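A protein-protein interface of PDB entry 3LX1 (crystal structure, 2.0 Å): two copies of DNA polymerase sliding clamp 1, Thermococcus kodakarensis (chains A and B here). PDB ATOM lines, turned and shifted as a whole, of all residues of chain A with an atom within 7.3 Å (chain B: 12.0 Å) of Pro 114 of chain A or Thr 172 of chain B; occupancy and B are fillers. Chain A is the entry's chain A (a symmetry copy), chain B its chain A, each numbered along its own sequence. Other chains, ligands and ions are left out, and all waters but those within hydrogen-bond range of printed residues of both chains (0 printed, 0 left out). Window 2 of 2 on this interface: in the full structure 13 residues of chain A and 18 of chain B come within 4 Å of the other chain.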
ATOM      1  N   GLY A  70      26.088 -16.623 -28.252  1.00  0.00           N
ATOM      2  CA  GLY A  70      26.283 -15.271 -27.786  1.00  0.00           C
ATOM      3  C   GLY A  70      24.941 -14.690 -27.466  1.00  0.00           C
ATOM      4  O   GLY A  70      23.967 -14.815 -28.242  1.00  0.00           O
ATOM      5  N   ILE A  71      24.879 -14.042 -26.321  1.00  0.00           N
ATOM      6  CA  ILE A  71      23.633 -13.664 -25.751  1.00  0.00           C
ATOM      7  C   ILE A  71      23.678 -12.202 -25.286  1.00  0.00           C
ATOM      8  O   ILE A  71      24.610 -11.790 -24.587  1.00  0.00           O
ATOM      9  CB  ILE A  71      23.271 -14.611 -24.531  1.00  0.00           C
ATOM     10  CG1 ILE A  71      22.709 -15.954 -25.051  1.00  0.00           C
ATOM     11  CG2 ILE A  71      22.182 -13.954 -23.683  1.00  0.00           C
ATOM     12  CD1 ILE A  71      22.348 -16.979 -23.993  1.00  0.00           C
ATOM     13  N   ASN A  72      22.689 -11.415 -25.699  1.00  0.00           N
ATOM     14  CA  ASN A  72      22.467 -10.113 -25.087  1.00  0.00           C
ATOM     15  C   ASN A  72      21.907 -10.302 -23.680  1.00  0.00           C
ATOM     16  O   ASN A  72      20.810 -10.810 -23.520  1.00  0.00           O
ATOM     17  CB  ASN A  72      21.527  -9.269 -25.967  1.00  0.00           C
ATOM     18  CG  ASN A  72      21.298  -7.875 -25.389  1.00  0.00           C
ATOM     19  OD1 ASN A  72      20.681  -7.704 -24.341  1.00  0.00           O
ATOM     20  ND2 ASN A  72      21.861  -6.892 -26.034  1.00  0.00           N
ATOM     21  N   GLN A  75      18.351  -8.587 -22.657  1.00  0.00           N
ATOM     22  CA  GLN A  75      17.226  -9.267 -23.319  1.00  0.00           C
ATOM     23  C   GLN A  75      16.970 -10.609 -22.678  1.00  0.00           C
ATOM     24  O   GLN A  75      15.808 -10.946 -22.371  1.00  0.00           O
ATOM     25  CB  GLN A  75      17.525  -9.453 -24.822  1.00  0.00           C
ATOM     26  CG  GLN A  75      17.582  -8.120 -25.631  1.00  0.00           C
ATOM     27  CD  GLN A  75      16.295  -7.245 -25.536  1.00  0.00           C
ATOM     28  OE1 GLN A  75      16.343  -6.092 -25.071  1.00  0.00           O
ATOM     29  NE2 GLN A  75      15.160  -7.785 -25.987  1.00  0.00           N
ATOM     30  N   ILE A  79      13.258 -11.643 -20.598  1.00  0.00           N
ATOM     31  CA  ILE A  79      12.498 -12.880 -20.812  1.00  0.00           C
ATOM     32  C   ILE A  79      12.478 -13.762 -19.587  1.00  0.00           C
ATOM     33  O   ILE A  79      11.392 -14.131 -19.094  1.00  0.00           O
ATOM     34  CB  ILE A  79      13.053 -13.667 -22.083  1.00  0.00           C
ATOM     35  CG1 ILE A  79      12.888 -12.825 -23.362  1.00  0.00           C
ATOM     36  CG2 ILE A  79      12.308 -14.986 -22.237  1.00  0.00           C
ATOM     37  CD1 ILE A  79      13.777 -13.394 -24.526  1.00  0.00           C
ATOM     38  N   ASN A  97      19.715 -19.698 -35.358  1.00  0.00           N
ATOM     39  CA  ASN A  97      20.455 -18.794 -34.429  1.00  0.00           C
ATOM     40  C   ASN A  97      19.519 -18.085 -33.439  1.00  0.00           C
ATOM     41  O   ASN A  97      19.490 -16.860 -33.325  1.00  0.00           O
ATOM     42  CB  ASN A  97      21.325 -17.764 -35.193  1.00  0.00           C
ATOM     43  CG  ASN A  97      22.572 -18.396 -35.822  1.00  0.00           C
ATOM     44  OD1 ASN A  97      23.214 -19.273 -35.217  1.00  0.00           O
ATOM     45  ND2 ASN A  97      22.941 -17.934 -37.029  1.00  0.00           N
ATOM     46  N   PHE A  98      18.697 -18.880 -32.781  1.00  0.00           N
ATOM     47  CA  PHE A  98      17.913 -18.411 -31.669  1.00  0.00           C
ATOM     48  C   PHE A  98      17.923 -19.482 -30.578  1.00  0.00           C
ATOM     49  O   PHE A  98      18.120 -20.666 -30.844  1.00  0.00           O
ATOM     50  CB  PHE A  98      16.491 -17.889 -32.048  1.00  0.00           C
ATOM     51  CG  PHE A  98      15.524 -18.959 -32.528  1.00  0.00           C
ATOM     52  CD1 PHE A  98      14.921 -19.852 -31.625  1.00  0.00           C
ATOM     53  CD2 PHE A  98      15.182 -19.028 -33.881  1.00  0.00           C
ATOM     54  CE1 PHE A  98      14.008 -20.843 -32.068  1.00  0.00           C
ATOM     55  CE2 PHE A  98      14.245 -19.990 -34.348  1.00  0.00           C
ATOM     56  CZ  PHE A  98      13.665 -20.913 -33.437  1.00  0.00           C
ATOM     57  N   LEU A  99      17.752 -19.011 -29.349  1.00  0.00           N
ATOM     58  CA  LEU A  99      17.608 -19.861 -28.204  1.00  0.00           C
ATOM     59  C   LEU A  99      16.123 -19.867 -27.908  1.00  0.00           C
ATOM     60  O   LEU A  99      15.494 -18.778 -27.840  1.00  0.00           O
ATOM     61  CB  LEU A  99      18.379 -19.225 -27.045  1.00  0.00           C
ATOM     62  CG  LEU A  99      18.279 -20.063 -25.757  1.00  0.00           C
ATOM     63  CD1 LEU A  99      18.959 -21.436 -25.931  1.00  0.00           C
ATOM     64  CD2 LEU A  99      18.891 -19.272 -24.547  1.00  0.00           C
ATOM     65  N   ARG A 112      11.430 -16.991 -28.257  1.00  0.00           N
ATOM     66  CA  ARG A 112      12.553 -17.070 -29.184  1.00  0.00           C
ATOM     67  C   ARG A 112      13.475 -15.862 -28.941  1.00  0.00           C
ATOM     68  O   ARG A 112      13.045 -14.706 -29.021  1.00  0.00           O
ATOM     69  CB  ARG A 112      12.047 -17.125 -30.640  1.00  0.00           C
ATOM     70  CG  ARG A 112      11.150 -18.378 -30.903  1.00  0.00           C
ATOM     71  CD  ARG A 112      10.433 -18.391 -32.288  1.00  0.00           C
ATOM     72  NE  ARG A 112      11.323 -18.678 -33.413  1.00  0.00           N
ATOM     73  CZ  ARG A 112      10.998 -18.564 -34.714  1.00  0.00           C
ATOM     74  NH1 ARG A 112       9.786 -18.164 -35.099  1.00  0.00           N
ATOM     75  NH2 ARG A 112      11.898 -18.857 -35.651  1.00  0.00           N
ATOM     76  N   LEU A 113      14.730 -16.132 -28.585  1.00  0.00           N
ATOM     77  CA  LEU A 113      15.698 -15.070 -28.382  1.00  0.00           C
ATOM     78  C   LEU A 113      16.750 -15.177 -29.473  1.00  0.00           C
ATOM     79  O   LEU A 113      17.491 -16.137 -29.503  1.00  0.00           O
ATOM     80  CB  LEU A 113      16.363 -15.187 -26.982  1.00  0.00           C
ATOM     81  CG  LEU A 113      17.530 -14.244 -26.588  1.00  0.00           C
ATOM     82  CD1 LEU A 113      17.061 -12.830 -26.126  1.00  0.00           C
ATOM     83  CD2 LEU A 113      18.485 -14.859 -25.549  1.00  0.00           C
ATOM     84  N   PRO A 114      16.837 -14.161 -30.353  1.00  0.00           N
ATOM     85  CA  PRO A 114      17.915 -14.109 -31.355  1.00  0.00           C
ATOM     86  C   PRO A 114      19.300 -14.125 -30.688  1.00  0.00           C
ATOM     87  O   PRO A 114      19.512 -13.461 -29.649  1.00  0.00           O
ATOM     88  CB  PRO A 114      17.728 -12.730 -32.011  1.00  0.00           C
ATOM     89  CG  PRO A 114      16.319 -12.335 -31.661  1.00  0.00           C
ATOM     90  CD  PRO A 114      16.041 -12.915 -30.319  1.00  0.00           C
ATOM     91  N   LEU A 115      20.240 -14.823 -31.289  1.00  0.00           N
ATOM     92  CA  LEU A 115      21.576 -14.819 -30.742  1.00  0.00           C
ATOM     93  C   LEU A 115      22.488 -13.891 -31.525  1.00  0.00           C
ATOM     94  O   LEU A 115      22.214 -13.553 -32.690  1.00  0.00           O
ATOM     95  CB  LEU A 115      22.140 -16.212 -30.712  1.00  0.00           C
ATOM     96  CG  LEU A 115      21.240 -17.210 -30.002  1.00  0.00           C
ATOM     97  CD1 LEU A 115      21.661 -18.589 -30.415  1.00  0.00           C
ATOM     98  CD2 LEU A 115      21.309 -17.005 -28.443  1.00  0.00           C
ATOM     99  N   ILE A 116      23.604 -13.514 -30.901  1.00  0.00           N
ATOM    100  CA  ILE A 116      24.487 -12.528 -31.498  1.00  0.00           C
ATOM    101  C   ILE A 116      25.917 -13.061 -31.541  1.00  0.00           C
ATOM    102  O   ILE A 116      26.238 -14.047 -30.875  1.00  0.00           O
ATOM    103  CB  ILE A 116      24.442 -11.200 -30.719  1.00  0.00           C
ATOM    104  CG1 ILE A 116      24.539 -11.492 -29.214  1.00  0.00           C
ATOM    105  CG2 ILE A 116      23.115 -10.406 -31.023  1.00  0.00           C
ATOM    106  CD1 ILE A 116      24.963 -10.332 -28.353  1.00  0.00           C
ATOM    107  N   ASP B 147       3.484 -11.938 -21.244  1.00  0.00           N
ATOM    108  CA  ASP B 147       4.547 -12.401 -22.140  1.00  0.00           C
ATOM    109  C   ASP B 147       4.509 -11.700 -23.464  1.00  0.00           C
ATOM    110  O   ASP B 147       5.544 -11.304 -23.969  1.00  0.00           O
ATOM    111  CB  ASP B 147       4.433 -13.902 -22.395  1.00  0.00           C
ATOM    112  CG  ASP B 147       4.579 -14.708 -21.124  1.00  0.00           C
ATOM    113  OD1 ASP B 147       4.992 -14.131 -20.081  1.00  0.00           O
ATOM    114  OD2 ASP B 147       4.223 -15.896 -21.153  1.00  0.00           O
ATOM    115  N   ALA B 148       3.304 -11.538 -24.036  1.00  0.00           N
ATOM    116  CA  ALA B 148       3.207 -10.968 -25.366  1.00  0.00           C
ATOM    117  C   ALA B 148       3.555  -9.471 -25.381  1.00  0.00           C
ATOM    118  O   ALA B 148       4.183  -8.980 -26.349  1.00  0.00           O
ATOM    119  CB  ALA B 148       1.757 -11.266 -26.023  1.00  0.00           C
ATOM    120  N   SER B 149       3.185  -8.761 -24.312  1.00  0.00           N
ATOM    121  CA  SER B 149       3.480  -7.332 -24.195  1.00  0.00           C
ATOM    122  C   SER B 149       4.953  -7.063 -24.126  1.00  0.00           C
ATOM    123  O   SER B 149       5.388  -6.007 -24.556  1.00  0.00           O
ATOM    124  CB  SER B 149       2.786  -6.669 -23.008  1.00  0.00           C
ATOM    125  OG  SER B 149       3.463  -6.999 -21.826  1.00  0.00           O
ATOM    126  N   LEU B 150       5.727  -8.029 -23.626  1.00  0.00           N
ATOM    127  CA  LEU B 150       7.198  -7.930 -23.672  1.00  0.00           C
ATOM    128  C   LEU B 150       7.667  -7.812 -25.103  1.00  0.00           C
ATOM    129  O   LEU B 150       8.628  -7.138 -25.406  1.00  0.00           O
ATOM    130  CB  LEU B 150       7.854  -9.181 -23.047  1.00  0.00           C
ATOM    131  CG  LEU B 150       9.290  -9.059 -22.557  1.00  0.00           C
ATOM    132  CD1 LEU B 150       9.276  -8.004 -21.441  1.00  0.00           C
ATOM    133  CD2 LEU B 150       9.805 -10.384 -22.024  1.00  0.00           C
ATOM    134  N   VAL B 151       6.963  -8.491 -25.992  1.00  0.00           N
ATOM    135  CA  VAL B 151       7.416  -8.753 -27.335  1.00  0.00           C
ATOM    136  C   VAL B 151       6.818  -7.834 -28.425  1.00  0.00           C
ATOM    137  O   VAL B 151       7.497  -7.494 -29.402  1.00  0.00           O
ATOM    138  CB  VAL B 151       7.042 -10.238 -27.608  1.00  0.00           C
ATOM    139  CG1 VAL B 151       6.866 -10.516 -29.050  1.00  0.00           C
ATOM    140  CG2 VAL B 151       8.038 -11.203 -26.889  1.00  0.00           C
ATOM    141  N   SER B 152       5.547  -7.444 -28.297  1.00  0.00           N
ATOM    142  CA  SER B 152       4.816  -6.838 -29.445  1.00  0.00           C
ATOM    143  C   SER B 152       3.731  -5.948 -28.877  1.00  0.00           C
ATOM    144  O   SER B 152       3.464  -5.998 -27.670  1.00  0.00           O
ATOM    145  CB  SER B 152       4.130  -7.960 -30.311  1.00  0.00           C
ATOM    146  OG  SER B 152       3.450  -7.436 -31.479  1.00  0.00           O
ATOM    147  N   ASP B 153       3.078  -5.172 -29.731  1.00  0.00           N
ATOM    148  CA  ASP B 153       1.869  -4.439 -29.346  1.00  0.00           C
ATOM    149  C   ASP B 153       0.624  -5.236 -29.766  1.00  0.00           C
ATOM    150  O   ASP B 153      -0.526  -4.790 -29.467  1.00  0.00           O
ATOM    151  CB  ASP B 153       1.781  -3.071 -30.059  1.00  0.00           C
ATOM    152  CG  ASP B 153       2.735  -2.017 -29.497  1.00  0.00           C
ATOM    153  OD1 ASP B 153       2.760  -1.816 -28.248  1.00  0.00           O
ATOM    154  OD2 ASP B 153       3.398  -1.332 -30.348  1.00  0.00           O
ATOM    155  N   ALA B 154       0.824  -6.320 -30.553  1.00  0.00           N
ATOM    156  CA  ALA B 154      -0.303  -7.181 -31.011  1.00  0.00           C
ATOM    157  C   ALA B 154      -0.203  -8.655 -30.638  1.00  0.00           C
ATOM    158  O   ALA B 154       0.872  -9.244 -30.612  1.00  0.00           O
ATOM    159  CB  ALA B 154      -0.591  -7.017 -32.552  1.00  0.00           C
ATOM    160  N   LYS B 167      -0.072 -16.018 -29.868  1.00  0.00           N
ATOM    161  CA  LYS B 167       1.214 -15.815 -30.499  1.00  0.00           C
ATOM    162  C   LYS B 167       1.434 -14.337 -30.664  1.00  0.00           C
ATOM    163  O   LYS B 167       0.496 -13.606 -30.988  1.00  0.00           O
ATOM    164  CB  LYS B 167       1.111 -16.483 -31.893  1.00  0.00           C
ATOM    165  CG  LYS B 167       2.368 -16.514 -32.691  1.00  0.00           C
ATOM    166  CD  LYS B 167       2.172 -17.426 -33.926  1.00  0.00           C
ATOM    167  CE  LYS B 167       1.678 -18.829 -33.525  1.00  0.00           C
ATOM    168  NZ  LYS B 167       1.788 -19.801 -34.679  1.00  0.00           N
ATOM    169  N   ALA B 168       2.679 -13.871 -30.481  1.00  0.00           N
ATOM    170  CA  ALA B 168       3.019 -12.482 -30.707  1.00  0.00           C
ATOM    171  C   ALA B 168       4.412 -12.410 -31.276  1.00  0.00           C
ATOM    172  O   ALA B 168       5.311 -13.246 -30.929  1.00  0.00           O
ATOM    173  CB  ALA B 168       2.952 -11.698 -29.406  1.00  0.00           C
ATOM    174  N   GLU B 169       4.616 -11.411 -32.141  1.00  0.00           N
ATOM    175  CA  GLU B 169       5.925 -11.241 -32.789  1.00  0.00           C
ATOM    176  C   GLU B 169       6.335  -9.793 -32.915  1.00  0.00           C
ATOM    177  O   GLU B 169       5.628  -9.001 -33.505  1.00  0.00           O
ATOM    178  CB  GLU B 169       5.935 -11.878 -34.171  1.00  0.00           C
ATOM    179  CG  GLU B 169       7.334 -11.857 -34.798  1.00  0.00           C
ATOM    180  CD  GLU B 169       7.500 -12.894 -35.897  1.00  0.00           C
ATOM    181  OE1 GLU B 169       6.496 -13.608 -36.221  1.00  0.00           O
ATOM    182  OE2 GLU B 169       8.640 -12.982 -36.437  1.00  0.00           O
ATOM    183  N   GLY B 170       7.490  -9.455 -32.349  1.00  0.00           N
ATOM    184  CA  GLY B 170       8.022  -8.110 -32.468  1.00  0.00           C
ATOM    185  C   GLY B 170       9.096  -8.102 -33.534  1.00  0.00           C
ATOM    186  O   GLY B 170       9.222  -9.062 -34.345  1.00  0.00           O
ATOM    187  N   GLU B 171       9.842  -7.010 -33.548  1.00  0.00           N
ATOM    188  CA  GLU B 171      10.952  -6.834 -34.449  1.00  0.00           C
ATOM    189  C   GLU B 171      11.955  -7.962 -34.219  1.00  0.00           C
ATOM    190  O   GLU B 171      12.308  -8.706 -35.152  1.00  0.00           O
ATOM    191  CB  GLU B 171      11.570  -5.446 -34.209  1.00  0.00           C
ATOM    192  CG  GLU B 171      11.996  -5.163 -32.756  1.00  0.00           C
ATOM    193  CD  GLU B 171      10.882  -5.315 -31.719  1.00  0.00           C
ATOM    194  OE1 GLU B 171       9.678  -5.319 -32.077  1.00  0.00           O
ATOM    195  OE2 GLU B 171      11.235  -5.410 -30.522  1.00  0.00           O
ATOM    196  N   THR B 172      12.338  -8.132 -32.955  1.00  0.00           N
ATOM    197  CA  THR B 172      13.376  -9.068 -32.577  1.00  0.00           C
ATOM    198  C   THR B 172      12.782 -10.320 -31.904  1.00  0.00           C
ATOM    199  O   THR B 172      13.008 -11.440 -32.373  1.00  0.00           O
ATOM    200  CB  THR B 172      14.388  -8.354 -31.690  1.00  0.00           C
ATOM    201  OG1 THR B 172      13.682  -7.530 -30.750  1.00  0.00           O
ATOM    202  CG2 THR B 172      15.263  -7.439 -32.549  1.00  0.00           C
ATOM    203  N   ASN B 173      12.014 -10.122 -30.833  1.00  0.00           N
ATOM    204  CA  ASN B 173      11.482 -11.213 -30.033  1.00  0.00           C
ATOM    205  C   ASN B 173      10.186 -11.851 -30.571  1.00  0.00           C
ATOM    206  O   ASN B 173       9.526 -11.304 -31.467  1.00  0.00           O
ATOM    207  CB  ASN B 173      11.303 -10.703 -28.594  1.00  0.00           C
ATOM    208  CG  ASN B 173      12.647 -10.538 -27.872  1.00  0.00           C
ATOM    209  OD1 ASN B 173      13.676 -11.139 -28.279  1.00  0.00           O
ATOM    210  ND2 ASN B 173      12.661  -9.704 -26.822  1.00  0.00           N
ATOM    211  N   GLU B 174       9.867 -13.029 -30.034  1.00  0.00           N
ATOM    212  CA  GLU B 174       8.655 -13.775 -30.364  1.00  0.00           C
ATOM    213  C   GLU B 174       8.260 -14.690 -29.194  1.00  0.00           C
ATOM    214  O   GLU B 174       9.138 -15.314 -28.553  1.00  0.00           O
ATOM    215  CB  GLU B 174       8.907 -14.622 -31.581  1.00  0.00           C
ATOM    216  CG  GLU B 174       7.675 -15.197 -32.121  1.00  0.00           C
ATOM    217  CD  GLU B 174       7.960 -16.423 -32.916  1.00  0.00           C
ATOM    218  OE1 GLU B 174       8.759 -16.292 -33.892  1.00  0.00           O
ATOM    219  OE2 GLU B 174       7.404 -17.496 -32.521  1.00  0.00           O
ATOM    220  N   VAL B 175       6.957 -14.755 -28.913  1.00  0.00           N
ATOM    221  CA  VAL B 175       6.427 -15.702 -27.935  1.00  0.00           C
ATOM    222  C   VAL B 175       5.226 -16.472 -28.500  1.00  0.00           C
ATOM    223  O   VAL B 175       4.479 -15.940 -29.350  1.00  0.00           O
ATOM    224  CB  VAL B 175       6.020 -15.027 -26.603  1.00  0.00           C
ATOM    225  CG1 VAL B 175       4.701 -14.240 -26.775  1.00  0.00           C
ATOM    226  CG2 VAL B 175       5.762 -16.067 -25.497  1.00  0.00           C
ATOM    227  N   GLU B 176       5.058 -17.696 -28.006  1.00  0.00           N
ATOM    228  CA  GLU B 176       3.907 -18.521 -28.280  1.00  0.00           C
ATOM    229  C   GLU B 176       3.487 -19.207 -26.984  1.00  0.00           C
ATOM    230  O   GLU B 176       4.315 -19.795 -26.269  1.00  0.00           O
ATOM    231  CB  GLU B 176       4.228 -19.479 -29.437  1.00  0.00           C
ATOM    232  CG  GLU B 176       3.276 -20.623 -29.661  1.00  0.00           C
ATOM    233  CD  GLU B 176       3.655 -21.442 -30.893  1.00  0.00           C
ATOM    234  OE1 GLU B 176       4.331 -20.891 -31.781  1.00  0.00           O
ATOM    235  OE2 GLU B 176       3.295 -22.645 -30.964  1.00  0.00           O
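No position is printed for both chains. Of the 6 pairs that touch across the chains among the printed residues, none has its exchanged pair printed and touching as well.
The side-chain carboxylate (OE2) of Glu 171 of chain B is in hydrogen-bond range of the side-chain hydroxyl (OG1) of Thr 172 of chain B. OD1 of Asn 72 of chain A is in hydrogen-bond range of N of Gln 75 of chain A (3.0 Å).
CA of Ile 79 of chain A touches CD2 of Leu 150 of chain B, at 3.9 Å. O of Arg 112 of chain A touches OD1 of Asn 173 of chain B, at 3.7 Å. Thr 172 of chain B touches Pro 114 of chain A (O to CG, 3.5 Å). Pro 114 of chain A touches Asn 173 of chain B.
No residue of chain B comes within 4 Å of Gly 70 of chain A. Ile 71 of chain A touches none of the printed residues of chain B. No residue of chain B comes within 4 Å of Asn 72 of chain A. Printed residues of chain B within 4 Å of Gln 75 of chain A: Asn 173. Of chain B, only Thr 172 (3.5 Å) and Asn 173 (3.6 Å) come within 4 Å of Pro 114 of chain A. No residue of chain B comes within 4 Å of Leu 115 of chain A. No residue of chain B comes within 4 Å of Ile 116 of chain A. Thr 172 of chain B touches one residue of chain A. Of the printed residues of chain A, Asn 173 of chain B touches Gln 75 (3.3 Å), Arg 112 (3.7 Å) and Pro 114 (3.6 Å).
The side-chain amide nitrogen of Gln 75 of chain A lies close to the side-chain amide nitrogen of Asn 173 of chain B. The guanidinium group of Arg 112 of chain A lies within salt-bridge range of the side-chain carboxylate of Glu 174 of chain B.
Of the 13 printed residues of chain A, 4 touch a printed residue of chain B. Printed residues of chain A that touch a printed residue of chain B: Gln 75, Ile 79, Arg 112 and Pro 114. Hydrophobic or aromatic side chains of chain A within 4 Å of the printed part of chain B: Pro 114. Along chain A the printed residues that touch a printed residue of chain B span positions 75 to 114. Hydrophobic or aromatic side chains of chain B within 4 Å of the printed part of chain A: Leu 150. Among the printed residues, Asp or Glu carboxylates within 4 Å of a Lys or Arg side-chain nitrogen of the other chain: Arg 112 of chain A with Glu 174 of chain B (2.5 Å).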
